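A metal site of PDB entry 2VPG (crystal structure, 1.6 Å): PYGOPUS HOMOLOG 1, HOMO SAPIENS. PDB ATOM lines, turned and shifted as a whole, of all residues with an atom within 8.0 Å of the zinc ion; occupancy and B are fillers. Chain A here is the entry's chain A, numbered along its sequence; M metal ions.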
ATOM      1  N   GLY A   9      27.279 -11.967  27.500  1.00  0.00           N
ATOM      2  CA  GLY A   9      28.527 -12.393  28.169  1.00  0.00           C
ATOM      3  C   GLY A   9      29.684 -11.445  27.921  1.00  0.00           C
ATOM      4  O   GLY A   9      30.676 -11.433  28.674  1.00  0.00           O
ATOM      5  N   LEU A  23      24.268 -18.829  21.972  1.00  0.00           N
ATOM      6  CA  LEU A  23      24.505 -19.385  23.290  1.00  0.00           C
ATOM      7  C   LEU A  23      25.854 -20.113  23.350  1.00  0.00           C
ATOM      8  O   LEU A  23      26.158 -20.909  22.451  1.00  0.00           O
ATOM      9  CB  LEU A  23      23.358 -20.351  23.608  1.00  0.00           C
ATOM     10  CG  LEU A  23      23.376 -21.063  24.958  1.00  0.00           C
ATOM     11  CD1 LEU A  23      23.370 -20.093  26.139  1.00  0.00           C
ATOM     12  CD2 LEU A  23      22.145 -21.948  25.001  1.00  0.00           C
ATOM     13  N   CYS A  24      26.651 -19.835  24.376  1.00  0.00           N
ATOM     14  CA  CYS A  24      27.878 -20.606  24.607  1.00  0.00           C
ATOM     15  C   CYS A  24      27.488 -21.979  25.164  1.00  0.00           C
ATOM     16  O   CYS A  24      27.463 -22.181  26.387  1.00  0.00           O
ATOM     17  CB  CYS A  24      28.818 -19.889  25.573  1.00  0.00           C
ATOM     18  SG  CYS A  24      30.436 -20.736  25.813  1.00  0.00           S
ATOM     19  N   GLU A  25      27.175 -22.905  24.256  1.00  0.00           N
ATOM     20  CA  GLU A  25      26.780 -24.258  24.678  1.00  0.00           C
ATOM     21  C   GLU A  25      28.003 -25.055  25.094  1.00  0.00           C
ATOM     22  O   GLU A  25      27.898 -26.030  25.859  1.00  0.00           O
ATOM     23  CB  GLU A  25      25.978 -24.951  23.579  1.00  0.00           C
ATOM     24  CG  GLU A  25      24.604 -24.358  23.384  1.00  0.00           C
ATOM     25  CD  GLU A  25      23.882 -24.967  22.213  1.00  0.00           C
ATOM     26  OE1 GLU A  25      22.967 -25.799  22.437  1.00  0.00           O
ATOM     27  OE2 GLU A  25      24.231 -24.630  21.063  1.00  0.00           O
ATOM     28  N   ALA A  26      29.177 -24.614  24.642  1.00  0.00           N
ATOM     29  CA  ALA A  26      30.454 -25.245  24.981  1.00  0.00           C
ATOM     30  C   ALA A  26      30.722 -25.281  26.483  1.00  0.00           C
ATOM     31  O   ALA A  26      31.198 -26.297  26.996  1.00  0.00           O
ATOM     32  CB  ALA A  26      31.609 -24.547  24.271  1.00  0.00           C
ATOM     33  N   SER A  27      30.422 -24.194  27.184  1.00  0.00           N
ATOM     34  CA  SER A  27      30.631 -24.178  28.632  1.00  0.00           C
ATOM     35  C   SER A  27      29.718 -23.253  29.432  1.00  0.00           C
ATOM     36  O   SER A  27      28.834 -23.728  30.167  1.00  0.00           O
ATOM     37  CB  SER A  27      32.084 -23.872  28.978  1.00  0.00           C
ATOM     38  OG  SER A  27      32.368 -24.335  30.286  1.00  0.00           O
ATOM     39  N   CYS A  28      29.931 -21.949  29.310  1.00  0.00           N
ATOM     40  CA  CYS A  28      29.380 -21.010  30.292  1.00  0.00           C
ATOM     41  C   CYS A  28      27.886 -20.752  30.192  1.00  0.00           C
ATOM     42  O   CYS A  28      27.295 -20.195  31.122  1.00  0.00           O
ATOM     43  CB  CYS A  28      30.157 -19.688  30.312  1.00  0.00           C
ATOM     44  SG  CYS A  28      29.929 -18.619  28.856  1.00  0.00           S
ATOM     45  N   GLN A  29      27.272 -21.152  29.069  1.00  0.00           N
ATOM     46  CA  GLN A  29      25.816 -21.022  28.879  1.00  0.00           C
ATOM     47  C   GLN A  29      25.283 -19.577  28.936  1.00  0.00           C
ATOM     48  O   GLN A  29      24.077 -19.361  29.159  1.00  0.00           O
ATOM     49  CB  GLN A  29      25.038 -21.903  29.870  1.00  0.00           C
ATOM     50  CG  GLN A  29      25.461 -23.369  29.950  1.00  0.00           C
ATOM     51  CD  GLN A  29      25.521 -24.089  28.596  1.00  0.00           C
ATOM     52  OE1 GLN A  29      24.658 -23.899  27.739  1.00  0.00           O
ATOM     53  NE2 GLN A  29      26.544 -24.920  28.420  1.00  0.00           N
ATOM     54  N   LYS A  30      26.171 -18.605  28.732  1.00  0.00           N
ATOM     55  CA  LYS A  30      25.701 -17.225  28.543  1.00  0.00           C
ATOM     56  C   LYS A  30      25.318 -17.034  27.075  1.00  0.00           C
ATOM     57  O   LYS A  30      25.879 -17.684  26.179  1.00  0.00           O
ATOM     58  CB  LYS A  30      26.768 -16.201  28.956  1.00  0.00           C
ATOM     59  CG  LYS A  30      27.289 -16.309  30.392  1.00  0.00           C
ATOM     60  CD  LYS A  30      28.399 -15.289  30.614  1.00  0.00           C
ATOM     61  CE  LYS A  30      29.059 -15.465  31.979  1.00  0.00           C
ATOM     62  NZ  LYS A  30      30.372 -14.737  32.092  1.00  0.00           N
ATOM     63  N   TRP A  31      24.341 -16.153  26.820  1.00  0.00           N
ATOM     64  CA  TRP A  31      24.069 -15.651  25.475  1.00  0.00           C
ATOM     65  C   TRP A  31      25.017 -14.481  25.154  1.00  0.00           C
ATOM     66  O   TRP A  31      25.431 -13.765  26.046  1.00  0.00           O
ATOM     67  CB  TRP A  31      22.604 -15.194  25.384  1.00  0.00           C
ATOM     68  CG  TRP A  31      21.661 -16.326  25.231  1.00  0.00           C
ATOM     69  CD1 TRP A  31      21.029 -17.024  26.231  1.00  0.00           C
ATOM     70  CD2 TRP A  31      21.230 -16.911  23.995  1.00  0.00           C
ATOM     71  NE1 TRP A  31      20.226 -17.997  25.696  1.00  0.00           N
ATOM     72  CE2 TRP A  31      20.323 -17.949  24.323  1.00  0.00           C
ATOM     73  CE3 TRP A  31      21.496 -16.639  22.653  1.00  0.00           C
ATOM     74  CZ2 TRP A  31      19.693 -18.739  23.332  1.00  0.00           C
ATOM     75  CZ3 TRP A  31      20.880 -17.428  21.665  1.00  0.00           C
ATOM     76  CH2 TRP A  31      19.998 -18.472  22.016  1.00  0.00           C
ATOM     77  N   PHE A  32      25.381 -14.359  23.875  1.00  0.00           N
ATOM     78  CA  PHE A  32      26.298 -13.312  23.411  1.00  0.00           C
ATOM     79  C   PHE A  32      25.752 -12.747  22.124  1.00  0.00           C
ATOM     80  O   PHE A  32      25.400 -13.512  21.221  1.00  0.00           O
ATOM     81  CB  PHE A  32      27.666 -13.948  23.064  1.00  0.00           C
ATOM     82  CG  PHE A  32      28.448 -14.455  24.259  1.00  0.00           C
ATOM     83  CD1 PHE A  32      29.560 -13.745  24.726  1.00  0.00           C
ATOM     84  CD2 PHE A  32      28.122 -15.650  24.888  1.00  0.00           C
ATOM     85  CE1 PHE A  32      30.316 -14.234  25.826  1.00  0.00           C
ATOM     86  CE2 PHE A  32      28.857 -16.130  25.977  1.00  0.00           C
ATOM     87  CZ  PHE A  32      29.940 -15.424  26.448  1.00  0.00           C
ATOM     88  N   TRP A  55      28.800 -23.767  19.785  1.00  0.00           N
ATOM     89  CA  TRP A  55      29.749 -22.689  19.842  1.00  0.00           C
ATOM     90  C   TRP A  55      30.209 -22.466  21.272  1.00  0.00           C
ATOM     91  O   TRP A  55      29.429 -22.628  22.239  1.00  0.00           O
ATOM     92  CB  TRP A  55      29.111 -21.420  19.231  1.00  0.00           C
ATOM     93  CG  TRP A  55      29.924 -20.176  19.388  1.00  0.00           C
ATOM     94  CD1 TRP A  55      30.975 -19.772  18.596  1.00  0.00           C
ATOM     95  CD2 TRP A  55      29.769 -19.163  20.388  1.00  0.00           C
ATOM     96  NE1 TRP A  55      31.475 -18.566  19.058  1.00  0.00           N
ATOM     97  CE2 TRP A  55      30.755 -18.173  20.152  1.00  0.00           C
ATOM     98  CE3 TRP A  55      28.910 -18.997  21.487  1.00  0.00           C
ATOM     99  CZ2 TRP A  55      30.889 -17.028  20.946  1.00  0.00           C
ATOM    100  CZ3 TRP A  55      29.040 -17.825  22.291  1.00  0.00           C
ATOM    101  CH2 TRP A  55      30.029 -16.874  22.018  1.00  0.00           C
ATOM    102  N   GLY A  56      31.483 -22.148  21.408  1.00  0.00           N
ATOM    103  CA  GLY A  56      32.037 -21.656  22.669  1.00  0.00           C
ATOM    104  C   GLY A  56      32.658 -20.272  22.536  1.00  0.00           C
ATOM    105  O   GLY A  56      33.294 -19.974  21.525  1.00  0.00           O
ATOM    106  N   CYS A  57      32.479 -19.425  23.562  1.00  0.00           N
ATOM    107  CA  CYS A  57      33.041 -18.079  23.567  1.00  0.00           C
ATOM    108  C   CYS A  57      34.553 -18.152  23.746  1.00  0.00           C
ATOM    109  O   CYS A  57      35.091 -19.192  24.128  1.00  0.00           O
ATOM    110  CB  CYS A  57      32.429 -17.225  24.670  1.00  0.00           C
ATOM    111  SG  CYS A  57      32.906 -17.714  26.348  1.00  0.00           S
ATOM    112  N   ASP A  58      35.246 -17.052  23.465  1.00  0.00           N
ATOM    113  CA  ASP A  58      36.703 -17.050  23.490  1.00  0.00           C
ATOM    114  C   ASP A  58      37.296 -17.487  24.836  1.00  0.00           C
ATOM    115  O   ASP A  58      38.276 -18.238  24.872  1.00  0.00           O
ATOM    116  CB  ASP A  58      37.233 -15.672  23.067  1.00  0.00           C
ATOM    117  CG  ASP A  58      36.879 -15.320  21.626  1.00  0.00           C
ATOM    118  OD1 ASP A  58      36.462 -16.210  20.847  1.00  0.00           O
ATOM    119  OD2 ASP A  58      37.045 -14.137  21.250  1.00  0.00           O
ATOM    120  N   THR A  59      36.699 -17.024  25.946  1.00  0.00           N
ATOM    121  CA  THR A  59      37.109 -17.433  27.296  1.00  0.00           C
ATOM    122  C   THR A  59      36.994 -18.928  27.530  1.00  0.00           C
ATOM    123  O   THR A  59      37.932 -19.553  28.036  1.00  0.00           O
ATOM    124  CB  THR A  59      36.295 -16.715  28.365  1.00  0.00           C
ATOM    125  OG1 THR A  59      36.518 -15.316  28.240  1.00  0.00           O
ATOM    126  CG2 THR A  59      36.697 -17.180  29.779  1.00  0.00           C
ATOM    127  N   CYS A  60      35.849 -19.508  27.166  1.00  0.00           N
ATOM    128  CA  CYS A  60      35.576 -20.922  27.375  1.00  0.00           C
ATOM    129  C   CYS A  60      36.457 -21.789  26.496  1.00  0.00           C
ATOM    130  O   CYS A  60      36.961 -22.821  26.941  1.00  0.00           O
ATOM    131  CB  CYS A  60      34.101 -21.233  27.155  1.00  0.00           C
ATOM    132  SG  CYS A  60      33.067 -20.626  28.515  1.00  0.00           S
ATOM    133  N   MET A  61      36.673 -21.357  25.255  1.00  0.00           N
ATOM    134  CA  MET A  61      37.514 -22.118  24.325  1.00  0.00           C
ATOM    135  C   MET A  61      38.992 -22.087  24.737  1.00  0.00           C
ATOM    136  O   MET A  61      39.714 -23.067  24.529  1.00  0.00           O
ATOM    137  CB  MET A  61      37.337 -21.608  22.889  1.00  0.00           C
ATOM    138  CG  MET A  61      35.945 -21.872  22.319  1.00  0.00           C
ATOM    139  SD  MET A  61      35.447 -23.594  22.400  1.00  0.00           S
ATOM    140  CE  MET A  61      36.312 -24.292  20.998  1.00  0.00           C
ATOM    141  N   ASP A  63      40.068 -22.119  27.799  1.00  0.00           N
ATOM    142  CA  ASP A  63      40.189 -23.044  28.926  1.00  0.00           C
ATOM    143  C   ASP A  63      40.453 -24.465  28.443  1.00  0.00           C
ATOM    144  O   ASP A  63      39.829 -24.928  27.478  1.00  0.00           O
ATOM    145  CB  ASP A  63      38.914 -23.030  29.788  1.00  0.00           C
ATOM    146  CG  ASP A  63      38.656 -21.672  30.453  1.00  0.00           C
ATOM    147  OD1 ASP A  63      39.560 -20.813  30.511  1.00  0.00           O
ATOM    148  OD2 ASP A  63      37.507 -21.483  30.926  1.00  0.00           O
HETATM  149 ZN    ZN M   1      31.468 -19.400  27.265  1.00  0.00          ZN
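O of Lys 30 is in hydrogen-bond range of N of Cys 24. The side-chain sulfur (SG) of Cys 24 sits close to the backbone NH (N) of Ser 27, at 3.7 Å. The backbone NH (N) of Lys 30 sits close to the side-chain sulfur (SG) of Cys 28 (3.8 Å). O of Cys 24 is in hydrogen-bond range of N of Gln 29 (2.9 Å).
Along chain A the residues within 4 Å of the zinc ion span positions 24 to 60. The nearest printed residue that does not touch the zinc ion is Phe 32 (4.3 Å).
The zinc ion is bound by SG of Cys 24 (2.2 Å), SG of Cys 28 (2.3 Å), SG of Cys 60 (2.4 Å) and SG of Cys 57 (2.4 Å). The zinc ion has four donor atoms within binding distance.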
